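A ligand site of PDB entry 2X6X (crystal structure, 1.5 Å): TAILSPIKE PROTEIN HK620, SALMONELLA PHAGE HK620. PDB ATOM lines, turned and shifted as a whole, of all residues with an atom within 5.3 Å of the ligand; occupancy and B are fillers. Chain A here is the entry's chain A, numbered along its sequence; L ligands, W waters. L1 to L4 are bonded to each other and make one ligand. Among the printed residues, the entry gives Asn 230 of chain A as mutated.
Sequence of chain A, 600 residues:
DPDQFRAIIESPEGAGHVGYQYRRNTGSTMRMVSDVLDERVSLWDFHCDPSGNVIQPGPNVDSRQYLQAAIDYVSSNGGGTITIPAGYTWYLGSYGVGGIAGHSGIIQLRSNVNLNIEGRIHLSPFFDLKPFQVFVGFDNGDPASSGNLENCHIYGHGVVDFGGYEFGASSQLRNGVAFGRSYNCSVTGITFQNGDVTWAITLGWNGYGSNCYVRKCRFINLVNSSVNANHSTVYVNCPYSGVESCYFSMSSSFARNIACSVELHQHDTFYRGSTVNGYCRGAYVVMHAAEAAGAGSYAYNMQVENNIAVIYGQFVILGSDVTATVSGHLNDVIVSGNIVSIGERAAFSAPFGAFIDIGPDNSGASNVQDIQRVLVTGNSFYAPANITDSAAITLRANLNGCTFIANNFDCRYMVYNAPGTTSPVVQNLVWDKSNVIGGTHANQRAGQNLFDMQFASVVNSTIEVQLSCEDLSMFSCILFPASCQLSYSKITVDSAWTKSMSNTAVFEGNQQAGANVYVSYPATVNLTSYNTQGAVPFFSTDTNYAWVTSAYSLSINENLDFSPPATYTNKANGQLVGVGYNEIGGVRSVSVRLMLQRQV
An oxygen (O1) of LG4 L4 lies within hydrogen-bond range of the side-chain amide oxygen (OD1) of Asn 206 (2.7 Å). A ring nitrogen (ND1) of His 103 is in hydrogen-bond range of an oxygen (O3) of LIG L1, at 2.7 Å. The side-chain amide nitrogen (ND2) of Asn 237 lies within hydrogen-bond range of an oxygen (O2) of LG4 L4 (2.9 Å). OE2 of Glu 291 sits at hydrogen-bond distance from N1 of LG4 L4 (2.9 Å). O3 of LIG L1 lies within hydrogen-bond range of NE2 of Gln 133. The side-chain hydroxyl (OH) of Tyr 235 lies within hydrogen-bond range of an oxygen (O2) of LG3 L3, 3.1 Å away. The side-chain amide nitrogen of Asn 230 sits at hydrogen-bond distance from an oxygen (O6) of LG3 L3 (3.4 Å).
The backbone NH (N) of Asn 206 lies close to the side-chain amide nitrogen (ND2) of Asn 237 (3.1 Å). NE2 of Gln 133 lies within hydrogen-bond range of O of His 103, 3.1 Å away. The side-chain carboxylate of Glu 291 is in hydrogen-bond range of the side-chain hydroxyl of Tyr 235.
Gly 102 touches the ligand. CZ of Phe 138 touches C6 of LIG L1 (3.9 Å). CD1 of Leu 173 touches O5 of LG2 L2, at 3.7 Å. CG2 of Thr 198 touches O6 of LG3 L3 (3.3 Å). Trp 199 touches the ligand. CG2 of Thr 202 touches C6 of LG4 L4, 3.7 Å away. NE1 of Trp 205 touches O1 of LG4 L4, at 3.6 Å. CB of Ala 290 touches C8 of LG4 L4, at 3.7 Å. Hydrophobic or aromatic side chains that line the ligand: His 103, Phe 138, Leu 173, Trp 199, Trp 205, Tyr 235 and Ala 290. Within 4 Å of the ligand: Gly 102, His 103, Gln 133, Phe 138, Leu 173, Thr 198, Trp 199, Thr 202, Trp 205, Asn 206, Asn 230, Tyr 235, Asn 237, Ala 290 and Glu 291. Along chain A the residues within 4 Å of the ligand span positions 102 to 291. The nearest printed residue that does not touch the ligand is His 288 (4.03 Å).
Water W1 lies within hydrogen-bond range of O2 of LG4 L4 (2.7 Å) and O of Gly 204 (2.8 Å). Water W5 bridges an oxygen (O1) of LIG L1 (2.7 Å) and the backbone carbonyl oxygen of Gly 102 (2.8 Å). Water W3 lies within hydrogen-bond range of an oxygen (O3) of LIG L1 (2.7 Å) and the side-chain amide oxygen (OE1) of Gln 133 (2.7 Å). Water W11 bridges the side-chain hydroxyl (OG1) of Thr 202 (2.7 Å) and an oxygen (O4) of LG4 L4 (2.7 Å). Water W9 lies within hydrogen-bond range of OE1 of Glu 263 (2.7 Å), O1 of LG3 L3 (2.8 Å) and NE2 of His 288 (3.2 Å). Water W10 bridges an oxygen (O4) of LIG L1 (2.9 Å) and the indole nitrogen of Trp 205 (3.1 Å).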
ATOM      1  N   GLY A 102      -6.171   9.970 -17.246  1.00  0.00           N
ATOM      2  CA  GLY A 102      -6.727   9.825 -15.900  1.00  0.00           C
ATOM      3  C   GLY A 102      -8.144   9.255 -15.866  1.00  0.00           C
ATOM      4  O   GLY A 102      -8.639   8.888 -14.785  1.00  0.00           O
ATOM      5  N   HIS A 103      -8.776   9.161 -17.028  1.00  0.00           N
ATOM      6  CA  HIS A 103     -10.124   8.629 -17.160  1.00  0.00           C
ATOM      7  C   HIS A 103     -10.106   7.304 -17.914  1.00  0.00           C
ATOM      8  O   HIS A 103     -11.151   6.843 -18.372  1.00  0.00           O
ATOM      9  CB  HIS A 103     -11.026   9.631 -17.908  1.00  0.00           C
ATOM     10  CG  HIS A 103     -11.046  10.998 -17.302  1.00  0.00           C
ATOM     11  ND1 HIS A 103     -11.921  11.360 -16.302  1.00  0.00           N
ATOM     12  CD2 HIS A 103     -10.308  12.101 -17.564  1.00  0.00           C
ATOM     13  CE1 HIS A 103     -11.720  12.630 -15.980  1.00  0.00           C
ATOM     14  NE2 HIS A 103     -10.741  13.097 -16.722  1.00  0.00           N
ATOM     15  N   GLN A 133     -12.721   4.230 -20.940  1.00  0.00           N
ATOM     16  CA  GLN A 133     -13.821   5.119 -21.294  1.00  0.00           C
ATOM     17  C   GLN A 133     -13.582   5.517 -22.721  1.00  0.00           C
ATOM     18  O   GLN A 133     -12.593   6.182 -23.023  1.00  0.00           O
ATOM     19  CB  GLN A 133     -13.881   6.338 -20.370  1.00  0.00           C
ATOM     20  CG  GLN A 133     -14.154   5.926 -18.921  1.00  0.00           C
ATOM     21  CD  GLN A 133     -14.594   7.092 -18.042  1.00  0.00           C
ATOM     22  OE1 GLN A 133     -15.570   7.811 -18.337  1.00  0.00           O
ATOM     23  NE2 GLN A 133     -13.874   7.285 -16.924  1.00  0.00           N
ATOM     24  N   PHE A 138     -13.613  15.378 -21.140  1.00  0.00           N
ATOM     25  CA  PHE A 138     -12.727  16.100 -20.228  1.00  0.00           C
ATOM     26  C   PHE A 138     -11.390  16.318 -20.934  1.00  0.00           C
ATOM     27  O   PHE A 138     -10.995  15.510 -21.767  1.00  0.00           O
ATOM     28  CB  PHE A 138     -12.457  15.277 -18.970  1.00  0.00           C
ATOM     29  CG  PHE A 138     -13.671  15.018 -18.099  1.00  0.00           C
ATOM     30  CD1 PHE A 138     -14.199  16.026 -17.303  1.00  0.00           C
ATOM     31  CD2 PHE A 138     -14.228  13.742 -18.014  1.00  0.00           C
ATOM     32  CE1 PHE A 138     -15.286  15.768 -16.464  1.00  0.00           C
ATOM     33  CE2 PHE A 138     -15.281  13.497 -17.183  1.00  0.00           C
ATOM     34  CZ  PHE A 138     -15.810  14.516 -16.401  1.00  0.00           C
ATOM     35  N   PRO A 143     -11.255  16.235 -13.157  1.00  0.00           N
ATOM     36  CA  PRO A 143     -12.395  16.933 -13.759  1.00  0.00           C
ATOM     37  C   PRO A 143     -12.601  18.365 -13.252  1.00  0.00           C
ATOM     38  O   PRO A 143     -13.085  19.213 -14.008  1.00  0.00           O
ATOM     39  CB  PRO A 143     -13.581  16.029 -13.417  1.00  0.00           C
ATOM     40  CG  PRO A 143     -13.146  15.113 -12.370  1.00  0.00           C
ATOM     41  CD  PRO A 143     -11.640  14.998 -12.468  1.00  0.00           C
ATOM     42  N   LEU A 173     -13.660   1.084 -13.677  1.00  0.00           N
ATOM     43  CA  LEU A 173     -14.774   1.794 -14.294  1.00  0.00           C
ATOM     44  C   LEU A 173     -14.673   1.658 -15.805  1.00  0.00           C
ATOM     45  O   LEU A 173     -13.557   1.685 -16.364  1.00  0.00           O
ATOM     46  CB  LEU A 173     -14.760   3.267 -13.921  1.00  0.00           C
ATOM     47  CG  LEU A 173     -14.890   3.640 -12.443  1.00  0.00           C
ATOM     48  CD1 LEU A 173     -14.615   5.139 -12.262  1.00  0.00           C
ATOM     49  CD2 LEU A 173     -16.244   3.261 -11.865  1.00  0.00           C
ATOM     50  N   THR A 198     -19.749   0.157 -16.646  1.00  0.00           N
ATOM     51  CA  THR A 198     -20.363   0.892 -15.531  1.00  0.00           C
ATOM     52  C   THR A 198     -21.510   1.779 -16.025  1.00  0.00           C
ATOM     53  O   THR A 198     -22.562   1.838 -15.411  1.00  0.00           O
ATOM     54  CB  THR A 198     -19.343   1.790 -14.821  1.00  0.00           C
ATOM     55  OG1 THR A 198     -18.144   1.051 -14.497  1.00  0.00           O
ATOM     56  CG2 THR A 198     -19.930   2.366 -13.545  1.00  0.00           C
ATOM     57  N   TRP A 199     -21.252   2.477 -17.132  1.00  0.00           N
ATOM     58  CA  TRP A 199     -22.233   3.340 -17.829  1.00  0.00           C
ATOM     59  C   TRP A 199     -21.986   3.158 -19.331  1.00  0.00           C
ATOM     60  O   TRP A 199     -20.863   2.781 -19.731  1.00  0.00           O
ATOM     61  CB  TRP A 199     -22.044   4.819 -17.498  1.00  0.00           C
ATOM     62  CG  TRP A 199     -21.787   5.148 -16.046  1.00  0.00           C
ATOM     63  CD1 TRP A 199     -22.703   5.255 -15.054  1.00  0.00           C
ATOM     64  CD2 TRP A 199     -20.516   5.446 -15.447  1.00  0.00           C
ATOM     65  NE1 TRP A 199     -22.094   5.599 -13.875  1.00  0.00           N
ATOM     66  CE2 TRP A 199     -20.746   5.702 -14.086  1.00  0.00           C
ATOM     67  CE3 TRP A 199     -19.206   5.479 -15.934  1.00  0.00           C
ATOM     68  CZ2 TRP A 199     -19.717   6.016 -13.204  1.00  0.00           C
ATOM     69  CZ3 TRP A 199     -18.177   5.783 -15.066  1.00  0.00           C
ATOM     70  CH2 TRP A 199     -18.436   6.056 -13.704  1.00  0.00           C
ATOM     71  N   THR A 202     -22.317   9.119 -19.966  1.00  0.00           N
ATOM     72  CA  THR A 202     -22.488  10.056 -18.870  1.00  0.00           C
ATOM     73  C   THR A 202     -22.557  11.482 -19.458  1.00  0.00           C
ATOM     74  O   THR A 202     -21.835  11.809 -20.426  1.00  0.00           O
ATOM     75  CB  THR A 202     -21.392   9.932 -17.788  1.00  0.00           C
ATOM     76  OG1 THR A 202     -20.112  10.284 -18.314  1.00  0.00           O
ATOM     77  CG2 THR A 202     -21.339   8.505 -17.243  1.00  0.00           C
ATOM     78  N   GLY A 204     -22.469  15.585 -18.409  1.00  0.00           N
ATOM     79  CA  GLY A 204     -22.097  16.541 -17.366  1.00  0.00           C
ATOM     80  C   GLY A 204     -21.135  16.004 -16.325  1.00  0.00           C
ATOM     81  O   GLY A 204     -20.753  14.833 -16.340  1.00  0.00           O
ATOM     82  N   TRP A 205     -20.779  16.869 -15.389  1.00  0.00           N
ATOM     83  CA  TRP A 205     -19.923  16.502 -14.280  1.00  0.00           C
ATOM     84  C   TRP A 205     -20.298  17.369 -13.079  1.00  0.00           C
ATOM     85  O   TRP A 205     -20.109  18.571 -13.118  1.00  0.00           O
ATOM     86  CB  TRP A 205     -18.422  16.681 -14.602  1.00  0.00           C
ATOM     87  CG  TRP A 205     -17.614  16.409 -13.392  1.00  0.00           C
ATOM     88  CD1 TRP A 205     -17.386  15.188 -12.815  1.00  0.00           C
ATOM     89  CD2 TRP A 205     -16.999  17.369 -12.533  1.00  0.00           C
ATOM     90  NE1 TRP A 205     -16.647  15.332 -11.684  1.00  0.00           N
ATOM     91  CE2 TRP A 205     -16.398  16.658 -11.476  1.00  0.00           C
ATOM     92  CE3 TRP A 205     -16.898  18.754 -12.568  1.00  0.00           C
ATOM     93  CZ2 TRP A 205     -15.693  17.303 -10.467  1.00  0.00           C
ATOM     94  CZ3 TRP A 205     -16.200  19.398 -11.552  1.00  0.00           C
ATOM     95  CH2 TRP A 205     -15.598  18.667 -10.523  1.00  0.00           C
ATOM     96  N   ASN A 206     -20.884  16.743 -12.054  1.00  0.00           N
ATOM     97  CA  ASN A 206     -21.246  17.409 -10.792  1.00  0.00           C
ATOM     98  C   ASN A 206     -21.961  18.723 -11.006  1.00  0.00           C
ATOM     99  O   ASN A 206     -21.658  19.738 -10.406  1.00  0.00           O
ATOM    100  CB  ASN A 206     -20.009  17.551  -9.896  1.00  0.00           C
ATOM    101  CG  ASN A 206     -19.504  16.205  -9.414  1.00  0.00           C
ATOM    102  OD1 ASN A 206     -20.067  15.164  -9.765  1.00  0.00           O
ATOM    103  ND2 ASN A 206     -18.437  16.222  -8.634  1.00  0.00           N
ATOM    104  N   ASN A 230     -21.611  -2.319 -10.360  1.00  0.00           N
ATOM    105  CA  ASN A 230     -22.780  -1.448 -10.507  1.00  0.00           C
ATOM    106  C   ASN A 230     -22.875  -0.969 -11.936  1.00  0.00           C
ATOM    107  O   ASN A 230     -21.854  -0.790 -12.611  1.00  0.00           O
ATOM    108  CB  ASN A 230     -22.639  -0.251  -9.561  1.00  0.00           C
ATOM    109  CG  ASN A 230     -23.866   0.663  -9.578  1.00  0.00           C
ATOM    110  OD1 ASN A 230     -24.998   0.210  -9.623  1.00  0.00           O
ATOM    111  ND2 ASN A 230     -23.613   1.970  -9.533  1.00  0.00           N
ATOM    112  N   TYR A 235     -26.148   8.293 -17.205  1.00  0.00           N
ATOM    113  CA  TYR A 235     -26.036   9.052 -15.957  1.00  0.00           C
ATOM    114  C   TYR A 235     -26.089  10.537 -16.318  1.00  0.00           C
ATOM    115  O   TYR A 235     -25.184  11.058 -17.001  1.00  0.00           O
ATOM    116  CB  TYR A 235     -24.733   8.710 -15.237  1.00  0.00           C
ATOM    117  CG  TYR A 235     -24.627   9.065 -13.773  1.00  0.00           C
ATOM    118  CD1 TYR A 235     -24.420  10.374 -13.359  1.00  0.00           C
ATOM    119  CD2 TYR A 235     -24.677   8.075 -12.789  1.00  0.00           C
ATOM    120  CE1 TYR A 235     -24.293  10.692 -12.016  1.00  0.00           C
ATOM    121  CE2 TYR A 235     -24.536   8.385 -11.447  1.00  0.00           C
ATOM    122  CZ  TYR A 235     -24.344   9.693 -11.060  1.00  0.00           C
ATOM    123  OH  TYR A 235     -24.194   9.993  -9.711  1.00  0.00           O
ATOM    124  N   ASN A 237     -25.783  14.118 -15.252  1.00  0.00           N
ATOM    125  CA  ASN A 237     -25.181  14.903 -14.175  1.00  0.00           C
ATOM    126  C   ASN A 237     -24.993  16.390 -14.544  1.00  0.00           C
ATOM    127  O   ASN A 237     -24.116  17.076 -14.043  1.00  0.00           O
ATOM    128  CB  ASN A 237     -23.860  14.274 -13.713  1.00  0.00           C
ATOM    129  CG  ASN A 237     -23.562  14.546 -12.256  1.00  0.00           C
ATOM    130  OD1 ASN A 237     -24.360  15.139 -11.546  1.00  0.00           O
ATOM    131  ND2 ASN A 237     -22.406  14.093 -11.794  1.00  0.00           N
ATOM    132  N   GLU A 263     -29.910   7.463 -14.502  1.00  0.00           N
ATOM    133  CA  GLU A 263     -29.920   8.231 -13.258  1.00  0.00           C
ATOM    134  C   GLU A 263     -30.064   9.708 -13.609  1.00  0.00           C
ATOM    135  O   GLU A 263     -29.358  10.233 -14.491  1.00  0.00           O
ATOM    136  CB  GLU A 263     -28.688   8.022 -12.400  1.00  0.00           C
ATOM    137  CG  GLU A 263     -28.365   6.572 -12.153  1.00  0.00           C
ATOM    138  CD  GLU A 263     -27.456   6.359 -10.939  1.00  0.00           C
ATOM    139  OE1 GLU A 263     -27.498   7.158  -9.969  1.00  0.00           O
ATOM    140  OE2 GLU A 263     -26.698   5.363 -10.943  1.00  0.00           O
ATOM    141  N   HIS A 288     -27.418  14.158  -4.877  1.00  0.00           N
ATOM    142  CA  HIS A 288     -26.216  13.866  -4.097  1.00  0.00           C
ATOM    143  C   HIS A 288     -25.537  15.189  -3.776  1.00  0.00           C
ATOM    144  O   HIS A 288     -25.109  15.880  -4.682  1.00  0.00           O
ATOM    145  CB  HIS A 288     -25.221  13.031  -4.907  1.00  0.00           C
ATOM    146  CG  HIS A 288     -25.578  11.585  -5.063  1.00  0.00           C
ATOM    147  ND1 HIS A 288     -26.014  10.791  -4.022  1.00  0.00           N
ATOM    148  CD2 HIS A 288     -25.489  10.771  -6.141  1.00  0.00           C
ATOM    149  CE1 HIS A 288     -26.201   9.564  -4.465  1.00  0.00           C
ATOM    150  NE2 HIS A 288     -25.897   9.525  -5.749  1.00  0.00           N
ATOM    151  N   ALA A 290     -22.570  15.546  -2.806  1.00  0.00           N
ATOM    152  CA  ALA A 290     -21.240  15.481  -3.408  1.00  0.00           C
ATOM    153  C   ALA A 290     -21.200  15.943  -4.877  1.00  0.00           C
ATOM    154  O   ALA A 290     -20.108  16.168  -5.426  1.00  0.00           O
ATOM    155  CB  ALA A 290     -20.654  14.067  -3.282  1.00  0.00           C
ATOM    156  N   GLU A 291     -22.375  16.075  -5.510  1.00  0.00           N
ATOM    157  CA  GLU A 291     -22.485  16.502  -6.904  1.00  0.00           C
ATOM    158  C   GLU A 291     -23.081  17.917  -7.107  1.00  0.00           C
ATOM    159  O   GLU A 291     -23.426  18.289  -8.218  1.00  0.00           O
ATOM    160  CB  GLU A 291     -23.289  15.454  -7.687  1.00  0.00           C
ATOM    161  CG  GLU A 291     -22.667  14.074  -7.675  1.00  0.00           C
ATOM    162  CD  GLU A 291     -23.521  13.062  -8.406  1.00  0.00           C
ATOM    163  OE1 GLU A 291     -24.755  13.252  -8.471  1.00  0.00           O
ATOM    164  OE2 GLU A 291     -22.971  12.072  -8.891  1.00  0.00           O
ATOM    165  N   ASN A 362     -25.987   6.077   0.290  1.00  0.00           N
ATOM    166  CA  ASN A 362     -25.028   5.013  -0.054  1.00  0.00           C
ATOM    167  C   ASN A 362     -24.456   4.288   1.167  1.00  0.00           C
ATOM    168  O   ASN A 362     -24.138   3.102   1.091  1.00  0.00           O
ATOM    169  CB  ASN A 362     -23.875   5.548  -0.928  1.00  0.00           C
ATOM    170  CG  ASN A 362     -24.330   5.934  -2.347  1.00  0.00           C
ATOM    171  OD1 ASN A 362     -25.433   5.578  -2.767  1.00  0.00           O
ATOM    172  ND2 ASN A 362     -23.473   6.651  -3.068  1.00  0.00           N
HETATM  173  C1  LIG L   1     -14.368   9.416 -11.104  1.00  0.00           C
HETATM  174  C2  LIG L   1     -13.149   8.750 -11.742  1.00  0.00           C
HETATM  175  C3  LIG L   1     -13.273   8.655 -13.267  1.00  0.00           C
HETATM  176  C4  LIG L   1     -13.711   9.997 -13.851  1.00  0.00           C
HETATM  177  C5  LIG L   1     -14.985  10.508 -13.141  1.00  0.00           C
HETATM  178  C6  LIG L   1     -15.388  11.902 -13.605  1.00  0.00           C
HETATM  179  O1  LIG L   1     -12.044   9.528 -11.403  1.00  0.00           O
HETATM  180  O2  LIG L   1     -12.041   8.260 -13.868  1.00  0.00           O
HETATM  181  O3  LIG L   1     -13.901   9.815 -15.240  1.00  0.00           O
HETATM  182  O4  LIG L   1     -14.739  10.625 -11.747  1.00  0.00           O
HETATM  183  C1  LG2 L   2     -17.766   5.586  -9.279  1.00  0.00           C
HETATM  184  C2  LG2 L   2     -16.662   5.263  -8.277  1.00  0.00           C
HETATM  185  C3  LG2 L   2     -16.240   6.518  -7.516  1.00  0.00           C
HETATM  186  C4  LG2 L   2     -15.843   7.598  -8.510  1.00  0.00           C
HETATM  187  C5  LG2 L   2     -16.996   7.837  -9.498  1.00  0.00           C
HETATM  188  C6  LG2 L   2     -16.678   8.802 -10.632  1.00  0.00           C
HETATM  189  O1  LG2 L   2     -17.202   4.311  -7.390  1.00  0.00           O
HETATM  190  O2  LG2 L   2     -15.165   6.243  -6.633  1.00  0.00           O
HETATM  191  O3  LG2 L   2     -15.550   8.772  -7.810  1.00  0.00           O
HETATM  192  O4  LG2 L   2     -17.325   6.619 -10.127  1.00  0.00           O
HETATM  193  O5  LG2 L   2     -15.454   8.526 -11.147  1.00  0.00           O
HETATM  194  C1  LG3 L   3     -22.117   6.057  -7.347  1.00  0.00           C
HETATM  195  C2  LG3 L   3     -21.525   7.419  -7.666  1.00  0.00           C
HETATM  196  C3  LG3 L   3     -20.891   7.311  -9.060  1.00  0.00           C
HETATM  197  C4  LG3 L   3     -20.118   5.987  -9.272  1.00  0.00           C
HETATM  198  C5  LG3 L   3     -21.022   4.758  -9.027  1.00  0.00           C
HETATM  199  C6  LG3 L   3     -20.310   3.407  -9.025  1.00  0.00           C
HETATM  200  O1  LG3 L   3     -23.237   6.127  -8.209  1.00  0.00           O
HETATM  201  O2  LG3 L   3     -22.509   8.415  -7.627  1.00  0.00           O
HETATM  202  O3  LG3 L   3     -20.099   8.459  -9.253  1.00  0.00           O
HETATM  203  O4  LG3 L   3     -18.951   5.964  -8.609  1.00  0.00           O
HETATM  204  O5  LG3 L   3     -21.753   4.780  -7.801  1.00  0.00           O
HETATM  205  O6  LG3 L   3     -20.442   2.786 -10.264  1.00  0.00           O
HETATM  206  C1  LG4 L   4     -20.539   9.432 -10.066  1.00  0.00           C
HETATM  207  C2  LG4 L   4     -19.807  10.729  -9.710  1.00  0.00           C
HETATM  208  C3  LG4 L   4     -19.977  11.870 -10.722  1.00  0.00           C
HETATM  209  C4  LG4 L   4     -19.933  11.367 -12.156  1.00  0.00           C
HETATM  210  C5  LG4 L   4     -20.732  10.092 -12.311  1.00  0.00           C
HETATM  211  C6  LG4 L   4     -20.721   9.556 -13.738  1.00  0.00           C
HETATM  212  C7  LG4 L   4     -19.466  11.155  -7.334  1.00  0.00           C
HETATM  213  C8  LG4 L   4     -20.049  11.681  -6.059  1.00  0.00           C
HETATM  214  N1  LG4 L   4     -20.249  11.197  -8.405  1.00  0.00           N
HETATM  215  O1  LG4 L   4     -18.980  12.861 -10.505  1.00  0.00           O
HETATM  216  O2  LG4 L   4     -20.456  12.383 -12.987  1.00  0.00           O
HETATM  217  O3  LG4 L   4     -20.286   9.078 -11.414  1.00  0.00           O
HETATM  218  O4  LG4 L   4     -19.414   9.196 -14.115  1.00  0.00           O
HETATM  219  O5  LG4 L   4     -18.318  10.707  -7.360  1.00  0.00           O
HETATM  220  O   HOH W   1     -18.939  13.125 -15.053  1.00  0.00           O
HETATM  221  O   HOH W   2     -22.936   2.413 -12.289  1.00  0.00           O
HETATM  222  O   HOH W   3     -15.946  10.091 -16.949  1.00  0.00           O
HETATM  223  O   HOH W   4     -19.427  10.669  -2.910  1.00  0.00           O
HETATM  224  O   HOH W   5     -10.061  10.496 -12.916  1.00  0.00           O
HETATM  225  O   HOH W   6     -15.239   2.324  -7.858  1.00  0.00           O
HETATM  226  O   HOH W   7     -11.488   5.591 -15.018  1.00  0.00           O
HETATM  227  O   HOH W   8     -18.965   0.650 -10.321  1.00  0.00           O
HETATM  228  O   HOH W   9     -25.861   7.020  -7.779  1.00  0.00           O
HETATM  229  O   HOH W  10     -16.082  12.646 -10.231  1.00  0.00           O
HETATM  230  O   HOH W  11     -18.427  10.584 -16.271  1.00  0.00           O
